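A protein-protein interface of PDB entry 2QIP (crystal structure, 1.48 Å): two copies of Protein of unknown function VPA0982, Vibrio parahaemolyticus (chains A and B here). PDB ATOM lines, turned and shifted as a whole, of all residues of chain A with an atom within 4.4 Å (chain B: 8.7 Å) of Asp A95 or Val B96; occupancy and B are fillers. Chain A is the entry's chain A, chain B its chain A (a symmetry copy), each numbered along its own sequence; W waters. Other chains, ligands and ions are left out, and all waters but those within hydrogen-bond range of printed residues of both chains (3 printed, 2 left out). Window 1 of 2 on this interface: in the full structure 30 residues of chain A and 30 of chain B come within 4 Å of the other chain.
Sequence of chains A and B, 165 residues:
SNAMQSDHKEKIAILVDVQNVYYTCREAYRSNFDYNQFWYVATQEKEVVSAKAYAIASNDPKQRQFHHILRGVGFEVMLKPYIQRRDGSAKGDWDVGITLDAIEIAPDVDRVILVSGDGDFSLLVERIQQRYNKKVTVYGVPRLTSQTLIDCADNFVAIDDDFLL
OD1 of Asp A120 lies within salt-bridge range of NZ of Lys B80, at 2.6 Å.
The side-chain carboxylate (OD1) of Asp A93 is in hydrogen-bond range of the backbone NH (N) of Asp A95, at 2.9 Å.
The backbone carbonyl oxygen (O) of Asp A95 sits at hydrogen-bond distance from the side-chain hydroxyl (OG1) of Thr A99.
The side-chain carboxylate of Asp A118 sits at hydrogen-bond distance from the backbone NH of Asp A120.
The backbone carbonyl oxygen of Asp B93 sits at hydrogen-bond distance from the side-chain amino group of Lys B80 (2.7 Å).
The backbone NH of Asp B95 sits at hydrogen-bond distance from the side-chain carboxylate of Asp B93, at 2.9 Å.
The backbone carbonyl oxygen of Asp B95 lies within hydrogen-bond range of the side-chain hydroxyl of Thr B99 (2.7 Å).
Among the printed residues, pairs that only touch across the chains: Asp A93 with Asp B120 (3.7 Å), Trp A94 with Leu B123 (3.6 Å), Asp A95 with Val B96 (3.9 Å), Val A96 with Asp B95 (3.9 Å), Val A96 with Thr B99 (3.5 Å), Val A96 with Asp B120 (3.7 Å), Val A96 with Leu B124 (3.98 Å), Gly A97 with Leu B123 (3.9 Å), Thr A99 with Val B96 (3.5 Å), Thr A99 with Thr B99 (3.8 Å), Thr A99 with Leu B100 (3.5 Å), Asp A120 with Ile B83 (3.5 Å), Asp A120 with Asp B93 (3.7 Å), Asp A120 with Val B96 (3.7 Å), Leu A123 with Ile B83 (3.8 Å), Leu A123 with Trp B94 (3.6 Å), Leu A123 with Gly B97 (3.9 Å), Leu A123 with Leu B100 (3.5 Å) and Leu A124 with Val B96 (3.98 Å).
Of the printed residues of chain B, Asp A93 touches Asp B120 (3.7 Å).
Of chain B, only Val B96 (3.9 Å) comes within 4 Å of Asp A95.
Of the printed residues of chain B, Gly A97 touches Leu B123 (3.9 Å).
Printed residues of chain A within 4 Å of Trp B94: Leu A123 (3.6 Å).
Of the printed residues of chain A, Asp B95 touches Val A96.
Among the printed residues, 20 pairs touch across the chains.
Asp A93 touches Asp B120, and with the chains exchanged Asp A120 touches Asp B93.
Asp A95 touches Val B96, and with the chains exchanged Val A96 touches Asp B95.
Val A96 touches Leu B124, and with the chains exchanged Leu A124 touches Val B96.
Thr A99 touches its own counterpart, Thr B99.
Positions printed for both chains: 93, 94, 95, 96, 97, 98, 99, 118, 120, 121, 123 and 124.
Of the 20 pairs that touch across the chains among the printed residues, 15 have their exchanged pair printed and touching as well.
Water W1 lies within hydrogen-bond range of the side-chain carboxylate (OD1) of Asp A93 (2.8 Å), the backbone NH (N) of Val A96 (3.0 Å), the side-chain carboxylate (OD2) of Asp B120 (3.3 Å) and the backbone NH (N) of Asp A95 (3.3 Å).
Water W2 lies within hydrogen-bond range of the side-chain carboxylate of Asp B93, the backbone NH of Val B96, the side-chain carboxylate of Asp A120 and the backbone NH of Asp B95.
Water W3 bridges OG of Ser B89 and OD1 of Asp A118.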
ATOM      1  N   ASP A  93     -30.170  22.127   8.296  1.00  0.00           N
ATOM      2  CA  ASP A  93     -28.830  22.010   8.901  1.00  0.00           C
ATOM      3  C   ASP A  93     -28.383  20.718   9.616  1.00  0.00           C
ATOM      4  O   ASP A  93     -29.028  20.190  10.527  1.00  0.00           O
ATOM      5  CB  ASP A  93     -28.119  23.361   9.167  1.00  0.00           C
ATOM      6  CG  ASP A  93     -27.569  23.540  10.561  1.00  0.00           C
ATOM      7  OD1 ASP A  93     -27.224  22.586  11.277  1.00  0.00           O
ATOM      8  OD2 ASP A  93     -27.442  24.734  10.928  1.00  0.00           O
ATOM      9  N   TRP A  94     -27.253  20.221   9.149  1.00  0.00           N
ATOM     10  CA  TRP A  94     -26.705  18.950   9.608  1.00  0.00           C
ATOM     11  C   TRP A  94     -25.617  19.130  10.680  1.00  0.00           C
ATOM     12  O   TRP A  94     -24.892  18.189  10.987  1.00  0.00           O
ATOM     13  CB  TRP A  94     -26.116  18.187   8.418  1.00  0.00           C
ATOM     14  CG  TRP A  94     -26.905  17.018   7.905  1.00  0.00           C
ATOM     15  CD1 TRP A  94     -27.465  16.885   6.652  1.00  0.00           C
ATOM     16  CD2 TRP A  94     -27.163  15.790   8.591  1.00  0.00           C
ATOM     17  NE1 TRP A  94     -28.075  15.663   6.539  1.00  0.00           N
ATOM     18  CE2 TRP A  94     -27.896  14.961   7.707  1.00  0.00           C
ATOM     19  CE3 TRP A  94     -26.847  15.302   9.875  1.00  0.00           C
ATOM     20  CZ2 TRP A  94     -28.291  13.664   8.060  1.00  0.00           C
ATOM     21  CZ3 TRP A  94     -27.248  14.023  10.225  1.00  0.00           C
ATOM     22  CH2 TRP A  94     -27.976  13.216   9.323  1.00  0.00           C
ATOM     23  N   ASP A  95     -25.489  20.317  11.261  1.00  0.00           N
ATOM     24  CA  ASP A  95     -24.387  20.537  12.198  1.00  0.00           C
ATOM     25  C   ASP A  95     -24.408  19.604  13.403  1.00  0.00           C
ATOM     26  O   ASP A  95     -23.358  19.130  13.832  1.00  0.00           O
ATOM     27  CB  ASP A  95     -24.299  21.996  12.654  1.00  0.00           C
ATOM     28  CG  ASP A  95     -23.922  22.951  11.516  1.00  0.00           C
ATOM     29  OD1 ASP A  95     -23.883  22.535  10.335  1.00  0.00           O
ATOM     30  OD2 ASP A  95     -23.653  24.143  11.830  1.00  0.00           O
ATOM     31  N   VAL A  96     -25.583  19.396  13.996  1.00  0.00           N
ATOM     32  CA  VAL A  96     -25.658  18.508  15.157  1.00  0.00           C
ATOM     33  C   VAL A  96     -25.210  17.087  14.761  1.00  0.00           C
ATOM     34  O   VAL A  96     -24.375  16.481  15.430  1.00  0.00           O
ATOM     35  CB  VAL A  96     -27.071  18.486  15.828  1.00  0.00           C
ATOM     36  CG1 VAL A  96     -27.146  17.365  16.875  1.00  0.00           C
ATOM     37  CG2 VAL A  96     -27.376  19.860  16.477  1.00  0.00           C
ATOM     38  N   GLY A  97     -25.737  16.558  13.655  1.00  0.00           N
ATOM     39  CA  GLY A  97     -25.422  15.176  13.320  1.00  0.00           C
ATOM     40  C   GLY A  97     -23.977  14.966  12.874  1.00  0.00           C
ATOM     41  O   GLY A  97     -23.357  13.948  13.199  1.00  0.00           O
ATOM     42  N   ILE A  98     -23.422  15.936  12.151  1.00  0.00           N
ATOM     43  CA  ILE A  98     -22.009  15.885  11.763  1.00  0.00           C
ATOM     44  C   ILE A  98     -21.106  15.953  13.001  1.00  0.00           C
ATOM     45  O   ILE A  98     -20.123  15.194  13.105  1.00  0.00           O
ATOM     46  CB  ILE A  98     -21.689  17.006  10.728  1.00  0.00           C
ATOM     47  CG1 ILE A  98     -22.331  16.637   9.377  1.00  0.00           C
ATOM     48  CG2 ILE A  98     -20.162  17.200  10.550  1.00  0.00           C
ATOM     49  CD1 ILE A  98     -22.269  17.759   8.311  1.00  0.00           C
ATOM     50  N   THR A  99     -21.462  16.820  13.956  1.00  0.00           N
ATOM     51  CA  THR A  99     -20.712  16.926  15.194  1.00  0.00           C
ATOM     52  C   THR A  99     -20.720  15.596  15.942  1.00  0.00           C
ATOM     53  O   THR A  99     -19.664  15.120  16.386  1.00  0.00           O
ATOM     54  CB  THR A  99     -21.239  18.073  16.062  1.00  0.00           C
ATOM     55  OG1 THR A  99     -21.090  19.292  15.329  1.00  0.00           O
ATOM     56  CG2 THR A  99     -20.480  18.205  17.380  1.00  0.00           C
ATOM     57  N   ASP A 118     -18.472  25.957   6.918  1.00  0.00           N
ATOM     58  CA  ASP A 118     -19.222  26.528   8.042  1.00  0.00           C
ATOM     59  C   ASP A 118     -18.335  26.701   9.285  1.00  0.00           C
ATOM     60  O   ASP A 118     -17.872  25.719   9.886  1.00  0.00           O
ATOM     61  CB  ASP A 118     -20.416  25.601   8.320  1.00  0.00           C
ATOM     62  CG  ASP A 118     -21.350  26.093   9.426  1.00  0.00           C
ATOM     63  OD1 ASP A 118     -20.991  26.993  10.214  1.00  0.00           O
ATOM     64  OD2 ASP A 118     -22.479  25.513   9.510  1.00  0.00           O
ATOM     65  N   ASP A 120     -18.941  27.361  12.257  1.00  0.00           N
ATOM     66  CA  ASP A 120     -19.355  26.767  13.530  1.00  0.00           C
ATOM     67  C   ASP A 120     -18.638  25.445  13.797  1.00  0.00           C
ATOM     68  O   ASP A 120     -18.521  25.012  14.942  1.00  0.00           O
ATOM     69  CB  ASP A 120     -20.864  26.600  13.627  1.00  0.00           C
ATOM     70  CG  ASP A 120     -21.558  27.881  14.045  1.00  0.00           C
ATOM     71  OD1 ASP A 120     -20.905  28.689  14.737  1.00  0.00           O
ATOM     72  OD2 ASP A 120     -22.739  28.080  13.673  1.00  0.00           O
ATOM     73  N   PHE A 121     -18.154  24.810  12.736  1.00  0.00           N
ATOM     74  CA  PHE A 121     -17.406  23.560  12.933  1.00  0.00           C
ATOM     75  C   PHE A 121     -16.015  23.786  13.554  1.00  0.00           C
ATOM     76  O   PHE A 121     -15.333  22.813  13.929  1.00  0.00           O
ATOM     77  CB  PHE A 121     -17.309  22.754  11.646  1.00  0.00           C
ATOM     78  CG  PHE A 121     -18.601  22.114  11.222  1.00  0.00           C
ATOM     79  CD1 PHE A 121     -19.302  21.282  12.087  1.00  0.00           C
ATOM     80  CD2 PHE A 121     -19.111  22.326   9.945  1.00  0.00           C
ATOM     81  CE1 PHE A 121     -20.520  20.680  11.674  1.00  0.00           C
ATOM     82  CE2 PHE A 121     -20.293  21.726   9.543  1.00  0.00           C
ATOM     83  CZ  PHE A 121     -21.013  20.903  10.393  1.00  0.00           C
ATOM     84  N   LEU A 123     -15.414  24.702  16.477  1.00  0.00           N
ATOM     85  CA  LEU A 123     -15.421  24.107  17.809  1.00  0.00           C
ATOM     86  C   LEU A 123     -15.227  22.598  17.748  1.00  0.00           C
ATOM     87  O   LEU A 123     -14.620  21.991  18.654  1.00  0.00           O
ATOM     88  CB  LEU A 123     -16.696  24.431  18.579  1.00  0.00           C
ATOM     89  CG  LEU A 123     -16.741  25.809  19.265  1.00  0.00           C
ATOM     90  CD1 LEU A 123     -16.772  26.949  18.256  1.00  0.00           C
ATOM     91  CD2 LEU A 123     -17.938  25.894  20.194  1.00  0.00           C
ATOM     92  N   LEU A 124     -15.740  21.997  16.681  1.00  0.00           N
ATOM     93  CA  LEU A 124     -15.600  20.551  16.485  1.00  0.00           C
ATOM     94  C   LEU A 124     -14.157  20.187  16.152  1.00  0.00           C
ATOM     95  O   LEU A 124     -13.603  19.222  16.708  1.00  0.00           O
ATOM     96  CB  LEU A 124     -16.551  20.080  15.381  1.00  0.00           C
ATOM     97  CG  LEU A 124     -16.309  18.671  14.825  1.00  0.00           C
ATOM     98  CD1 LEU A 124     -16.476  17.587  15.903  1.00  0.00           C
ATOM     99  CD2 LEU A 124     -17.234  18.447  13.621  1.00  0.00           C
ATOM    100  N   LEU B  15     -27.948  22.190  30.273  1.00  0.00           N
ATOM    101  CA  LEU B  15     -27.386  22.984  29.172  1.00  0.00           C
ATOM    102  C   LEU B  15     -28.482  23.919  28.685  1.00  0.00           C
ATOM    103  O   LEU B  15     -29.540  23.449  28.246  1.00  0.00           O
ATOM    104  CB  LEU B  15     -26.923  22.112  28.007  1.00  0.00           C
ATOM    105  CG  LEU B  15     -25.729  21.185  28.285  1.00  0.00           C
ATOM    106  CD1 LEU B  15     -26.178  19.833  28.873  1.00  0.00           C
ATOM    107  CD2 LEU B  15     -24.946  20.983  26.992  1.00  0.00           C
ATOM    108  N   TYR B  54     -25.206  28.754  27.539  1.00  0.00           N
ATOM    109  CA  TYR B  54     -24.464  29.041  26.309  1.00  0.00           C
ATOM    110  C   TYR B  54     -24.986  30.345  25.727  1.00  0.00           C
ATOM    111  O   TYR B  54     -26.118  30.417  25.216  1.00  0.00           O
ATOM    112  CB  TYR B  54     -24.657  27.870  25.330  1.00  0.00           C
ATOM    113  CG  TYR B  54     -24.027  26.613  25.883  1.00  0.00           C
ATOM    114  CD1 TYR B  54     -22.740  26.256  25.514  1.00  0.00           C
ATOM    115  CD2 TYR B  54     -24.704  25.799  26.799  1.00  0.00           C
ATOM    116  CE1 TYR B  54     -22.120  25.123  26.029  1.00  0.00           C
ATOM    117  CE2 TYR B  54     -24.087  24.655  27.335  1.00  0.00           C
ATOM    118  CZ  TYR B  54     -22.798  24.315  26.926  1.00  0.00           C
ATOM    119  OH  TYR B  54     -22.161  23.190  27.456  1.00  0.00           O
ATOM    120  N   LYS B  80     -19.737  32.401  23.347  1.00  0.00           N
ATOM    121  CA  LYS B  80     -19.326  31.835  22.077  1.00  0.00           C
ATOM    122  C   LYS B  80     -18.000  32.438  21.602  1.00  0.00           C
ATOM    123  O   LYS B  80     -17.848  33.667  21.594  1.00  0.00           O
ATOM    124  CB  LYS B  80     -20.413  32.007  21.019  1.00  0.00           C
ATOM    125  CG  LYS B  80     -20.114  31.162  19.804  1.00  0.00           C
ATOM    126  CD  LYS B  80     -21.231  31.150  18.812  1.00  0.00           C
ATOM    127  CE  LYS B  80     -20.898  30.167  17.691  1.00  0.00           C
ATOM    128  NZ  LYS B  80     -21.864  30.300  16.589  1.00  0.00           N
ATOM    129  N   ILE B  83     -16.019  33.763  15.656  1.00  0.00           N
ATOM    130  CA  ILE B  83     -15.915  32.931  14.458  1.00  0.00           C
ATOM    131  C   ILE B  83     -16.089  33.841  13.260  1.00  0.00           C
ATOM    132  O   ILE B  83     -17.148  34.433  13.080  1.00  0.00           O
ATOM    133  CB  ILE B  83     -16.970  31.780  14.438  1.00  0.00           C
ATOM    134  CG1 ILE B  83     -16.695  30.772  15.576  1.00  0.00           C
ATOM    135  CG2 ILE B  83     -16.945  31.069  13.074  1.00  0.00           C
ATOM    136  CD1 ILE B  83     -17.728  29.691  15.762  1.00  0.00           C
ATOM    137  N   SER B  89     -23.958  33.774   6.800  1.00  0.00           N
ATOM    138  CA  SER B  89     -24.791  32.933   7.674  1.00  0.00           C
ATOM    139  C   SER B  89     -24.931  33.500   9.096  1.00  0.00           C
ATOM    140  O   SER B  89     -24.176  34.383   9.499  1.00  0.00           O
ATOM    141  CB  SER B  89     -24.217  31.515   7.734  1.00  0.00           C
ATOM    142  OG  SER B  89     -22.922  31.520   8.321  1.00  0.00           O
ATOM    143  N   ALA B  90     -25.896  32.970   9.850  1.00  0.00           N
ATOM    144  CA  ALA B  90     -26.171  33.411  11.223  1.00  0.00           C
ATOM    145  C   ALA B  90     -24.988  33.170  12.167  1.00  0.00           C
ATOM    146  O   ALA B  90     -24.476  32.050  12.253  1.00  0.00           O
ATOM    147  CB  ALA B  90     -27.421  32.718  11.748  1.00  0.00           C
ATOM    148  N   GLY B  92     -24.990  33.473  15.524  1.00  0.00           N
ATOM    149  CA  GLY B  92     -25.354  33.186  16.903  1.00  0.00           C
ATOM    150  C   GLY B  92     -25.514  31.738  17.332  1.00  0.00           C
ATOM    151  O   GLY B  92     -25.858  31.489  18.501  1.00  0.00           O
ATOM    152  N   ASP B  93     -25.285  30.768  16.442  1.00  0.00           N
ATOM    153  CA  ASP B  93     -25.671  29.402  16.839  1.00  0.00           C
ATOM    154  C   ASP B  93     -24.700  28.488  17.614  1.00  0.00           C
ATOM    155  O   ASP B  93     -23.554  28.236  17.230  1.00  0.00           O
ATOM    156  CB  ASP B  93     -26.874  28.815  16.057  1.00  0.00           C
ATOM    157  CG  ASP B  93     -26.656  27.443  15.469  1.00  0.00           C
ATOM    158  OD1 ASP B  93     -25.860  26.621  15.952  1.00  0.00           O
ATOM    159  OD2 ASP B  93     -27.378  27.173  14.478  1.00  0.00           O
ATOM    160  N   TRP B  94     -25.206  28.013  18.737  1.00  0.00           N
ATOM    161  CA  TRP B  94     -24.425  27.215  19.676  1.00  0.00           C
ATOM    162  C   TRP B  94     -24.657  25.705  19.502  1.00  0.00           C
ATOM    163  O   TRP B  94     -24.273  24.919  20.362  1.00  0.00           O
ATOM    164  CB  TRP B  94     -24.781  27.617  21.109  1.00  0.00           C
ATOM    165  CG  TRP B  94     -23.775  28.449  21.851  1.00  0.00           C
ATOM    166  CD1 TRP B  94     -23.953  29.730  22.328  1.00  0.00           C
ATOM    167  CD2 TRP B  94     -22.468  28.044  22.268  1.00  0.00           C
ATOM    168  NE1 TRP B  94     -22.825  30.146  22.985  1.00  0.00           N
ATOM    169  CE2 TRP B  94     -21.899  29.129  22.978  1.00  0.00           C
ATOM    170  CE3 TRP B  94     -21.713  26.865  22.109  1.00  0.00           C
ATOM    171  CZ2 TRP B  94     -20.623  29.055  23.551  1.00  0.00           C
ATOM    172  CZ3 TRP B  94     -20.446  26.798  22.668  1.00  0.00           C
ATOM    173  CH2 TRP B  94     -19.904  27.894  23.374  1.00  0.00           C
ATOM    174  N   ASP B  95     -25.275  25.280  18.407  1.00  0.00           N
ATOM    175  CA  ASP B  95     -25.606  23.861  18.279  1.00  0.00           C
ATOM    176  C   ASP B  95     -24.393  22.939  18.327  1.00  0.00           C
ATOM    177  O   ASP B  95     -24.454  21.874  18.938  1.00  0.00           O
ATOM    178  CB  ASP B  95     -26.447  23.573  17.033  1.00  0.00           C
ATOM    179  CG  ASP B  95     -27.843  24.203  17.100  1.00  0.00           C
ATOM    180  OD1 ASP B  95     -28.126  25.000  18.023  1.00  0.00           O
ATOM    181  OD2 ASP B  95     -28.667  23.874  16.203  1.00  0.00           O
ATOM    182  N   VAL B  96     -23.319  23.304  17.627  1.00  0.00           N
ATOM    183  CA  VAL B  96     -22.127  22.454  17.640  1.00  0.00           C
ATOM    184  C   VAL B  96     -21.585  22.333  19.078  1.00  0.00           C
ATOM    185  O   VAL B  96     -21.323  21.233  19.562  1.00  0.00           O
ATOM    186  CB  VAL B  96     -21.012  22.940  16.657  1.00  0.00           C
ATOM    187  CG1 VAL B  96     -19.714  22.156  16.896  1.00  0.00           C
ATOM    188  CG2 VAL B  96     -21.485  22.777  15.190  1.00  0.00           C
ATOM    189  N   GLY B  97     -21.440  23.457  19.782  1.00  0.00           N
ATOM    190  CA  GLY B  97     -20.821  23.386  21.098  1.00  0.00           C
ATOM    191  C   GLY B  97     -21.690  22.701  22.149  1.00  0.00           C
ATOM    192  O   GLY B  97     -21.185  21.968  23.007  1.00  0.00           O
ATOM    193  N   ILE B  98     -23.002  22.909  22.076  1.00  0.00           N
ATOM    194  CA  ILE B  98     -23.937  22.214  22.968  1.00  0.00           C
ATOM    195  C   ILE B  98     -23.912  20.703  22.705  1.00  0.00           C
ATOM    196  O   ILE B  98     -23.890  19.899  23.657  1.00  0.00           O
ATOM    197  CB  ILE B  98     -25.366  22.820  22.837  1.00  0.00           C
ATOM    198  CG1 ILE B  98     -25.382  24.213  23.497  1.00  0.00           C
ATOM    199  CG2 ILE B  98     -26.435  21.913  23.496  1.00  0.00           C
ATOM    200  CD1 ILE B  98     -26.684  25.018  23.260  1.00  0.00           C
ATOM    201  N   THR B  99     -23.866  20.318  21.424  1.00  0.00           N
ATOM    202  CA  THR B  99     -23.782  18.916  21.061  1.00  0.00           C
ATOM    203  C   THR B  99     -22.516  18.288  21.636  1.00  0.00           C
ATOM    204  O   THR B  99     -22.572  17.207  22.243  1.00  0.00           O
ATOM    205  CB  THR B  99     -23.874  18.731  19.544  1.00  0.00           C
ATOM    206  OG1 THR B  99     -25.136  19.243  19.107  1.00  0.00           O
ATOM    207  CG2 THR B  99     -23.776  17.266  19.127  1.00  0.00           C
ATOM    208  N   LEU B 100     -21.372  18.955  21.447  1.00  0.00           N
ATOM    209  CA  LEU B 100     -20.102  18.425  21.979  1.00  0.00           C
ATOM    210  C   LEU B 100     -20.174  18.208  23.496  1.00  0.00           C
ATOM    211  O   LEU B 100     -19.779  17.157  24.012  1.00  0.00           O
ATOM    212  CB  LEU B 100     -18.966  19.393  21.672  1.00  0.00           C
ATOM    213  CG  LEU B 100     -18.537  19.465  20.217  1.00  0.00           C
ATOM    214  CD1 LEU B 100     -17.580  20.640  20.070  1.00  0.00           C
ATOM    215  CD2 LEU B 100     -17.896  18.171  19.750  1.00  0.00           C
ATOM    216  N   ASP B 101     -20.652  19.220  24.209  1.00  0.00           N
ATOM    217  CA  ASP B 101     -20.648  19.171  25.671  1.00  0.00           C
ATOM    218  C   ASP B 101     -21.684  18.190  26.226  1.00  0.00           C
ATOM    219  O   ASP B 101     -21.422  17.537  27.251  1.00  0.00           O
ATOM    220  CB  ASP B 101     -20.883  20.578  26.251  1.00  0.00           C
ATOM    221  CG  ASP B 101     -19.663  21.480  26.146  1.00  0.00           C
ATOM    222  OD1 ASP B 101     -18.554  21.003  25.775  1.00  0.00           O
ATOM    223  OD2 ASP B 101     -19.832  22.685  26.475  1.00  0.00           O
ATOM    224  N   ALA B 102     -22.848  18.099  25.583  1.00  0.00           N
ATOM    225  CA  ALA B 102     -23.898  17.225  26.083  1.00  0.00           C
ATOM    226  C   ALA B 102     -23.445  15.769  25.980  1.00  0.00           C
ATOM    227  O   ALA B 102     -23.650  14.986  26.902  1.00  0.00           O
ATOM    228  CB  ALA B 102     -25.180  17.438  25.309  1.00  0.00           C
ATOM    229  N   ILE B 103     -22.827  15.405  24.854  1.00  0.00           N
ATOM    230  CA  ILE B 103     -22.295  14.026  24.752  1.00  0.00           C
ATOM    231  C   ILE B 103     -21.178  13.761  25.747  1.00  0.00           C
ATOM    232  O   ILE B 103     -21.105  12.668  26.343  1.00  0.00           O
ATOM    233  CB  ILE B 103     -21.794  13.730  23.343  1.00  0.00           C
ATOM    234  CG1 ILE B 103     -22.986  13.547  22.433  1.00  0.00           C
ATOM    235  CG2 ILE B 103     -20.863  12.489  23.312  1.00  0.00           C
ATOM    236  CD1 ILE B 103     -23.894  12.304  22.762  1.00  0.00           C
ATOM    237  N   GLU B 104     -20.297  14.749  25.941  1.00  0.00           N
ATOM    238  CA  GLU B 104     -19.230  14.591  26.917  1.00  0.00           C
ATOM    239  C   GLU B 104     -19.742  14.368  28.345  1.00  0.00           C
ATOM    240  O   GLU B 104     -19.158  13.591  29.110  1.00  0.00           O
ATOM    241  CB  GLU B 104     -18.258  15.772  26.862  1.00  0.00           C
ATOM    242  CG  GLU B 104     -17.209  15.617  25.796  1.00  0.00           C
ATOM    243  CD  GLU B 104     -16.268  16.802  25.770  1.00  0.00           C
ATOM    244  OE1 GLU B 104     -15.928  17.250  24.659  1.00  0.00           O
ATOM    245  OE2 GLU B 104     -15.916  17.308  26.858  1.00  0.00           O
ATOM    246  N   ASP B 118     -35.087  23.988  19.813  1.00  0.00           N
ATOM    247  CA  ASP B 118     -34.538  23.731  18.476  1.00  0.00           C
ATOM    248  C   ASP B 118     -34.575  22.236  18.127  1.00  0.00           C
ATOM    249  O   ASP B 118     -33.879  21.414  18.744  1.00  0.00           O
ATOM    250  CB  ASP B 118     -33.106  24.287  18.450  1.00  0.00           C
ATOM    251  CG  ASP B 118     -32.409  24.165  17.094  1.00  0.00           C
ATOM    252  OD1 ASP B 118     -32.862  23.411  16.207  1.00  0.00           O
ATOM    253  OD2 ASP B 118     -31.341  24.840  16.946  1.00  0.00           O
ATOM    254  N   ASP B 120     -33.310  20.550  15.847  1.00  0.00           N
ATOM    255  CA  ASP B 120     -32.080  19.874  15.432  1.00  0.00           C
ATOM    256  C   ASP B 120     -31.447  19.095  16.584  1.00  0.00           C
ATOM    257  O   ASP B 120     -30.682  18.157  16.366  1.00  0.00           O
ATOM    258  CB  ASP B 120     -31.078  20.830  14.802  1.00  0.00           C
ATOM    259  CG  ASP B 120     -31.378  21.094  13.340  1.00  0.00           C
ATOM    260  OD1 ASP B 120     -31.976  20.202  12.706  1.00  0.00           O
ATOM    261  OD2 ASP B 120     -31.028  22.189  12.839  1.00  0.00           O
ATOM    262  N   PHE B 121     -31.773  19.485  17.811  1.00  0.00           N
ATOM    263  CA  PHE B 121     -31.239  18.741  18.961  1.00  0.00           C
ATOM    264  C   PHE B 121     -31.883  17.351  19.126  1.00  0.00           C
ATOM    265  O   PHE B 121     -31.420  16.543  19.954  1.00  0.00           O
ATOM    266  CB  PHE B 121     -31.337  19.547  20.247  1.00  0.00           C
ATOM    267  CG  PHE B 121     -30.373  20.698  20.327  1.00  0.00           C
ATOM    268  CD1 PHE B 121     -29.008  20.496  20.159  1.00  0.00           C
ATOM    269  CD2 PHE B 121     -30.827  21.986  20.590  1.00  0.00           C
ATOM    270  CE1 PHE B 121     -28.106  21.591  20.241  1.00  0.00           C
ATOM    271  CE2 PHE B 121     -29.942  23.047  20.681  1.00  0.00           C
ATOM    272  CZ  PHE B 121     -28.579  22.871  20.505  1.00  0.00           C
ATOM    273  N   LEU B 123     -31.490  14.890  17.246  1.00  0.00           N
ATOM    274  CA  LEU B 123     -30.458  13.890  16.992  1.00  0.00           C
ATOM    275  C   LEU B 123     -29.557  13.695  18.203  1.00  0.00           C
ATOM    276  O   LEU B 123     -29.058  12.581  18.460  1.00  0.00           O
ATOM    277  CB  LEU B 123     -29.612  14.233  15.771  1.00  0.00           C
ATOM    278  CG  LEU B 123     -30.216  13.865  14.403  1.00  0.00           C
ATOM    279  CD1 LEU B 123     -31.451  14.695  14.081  1.00  0.00           C
ATOM    280  CD2 LEU B 123     -29.175  14.022  13.310  1.00  0.00           C
ATOM    281  N   LEU B 124     -29.353  14.776  18.946  1.00  0.00           N
ATOM    282  CA  LEU B 124     -28.528  14.721  20.156  1.00  0.00           C
ATOM    283  C   LEU B 124     -29.238  13.944  21.260  1.00  0.00           C
ATOM    284  O   LEU B 124     -28.625  13.094  21.930  1.00  0.00           O
ATOM    285  CB  LEU B 124     -28.186  16.140  20.620  1.00  0.00           C
ATOM    286  CG  LEU B 124     -27.611  16.276  22.035  1.00  0.00           C
ATOM    287  CD1 LEU B 124     -26.272  15.537  22.189  1.00  0.00           C
ATOM    288  CD2 LEU B 124     -27.499  17.767  22.384  1.00  0.00           C
HETATM  289  O   HOH W   1     -28.045  20.918  13.317  1.00  0.00           O
HETATM  290  O   HOH W   2     -23.307  25.594  15.732  1.00  0.00           O
HETATM  291  O   HOH W   3     -21.905  29.885  10.694  1.00  0.00           O
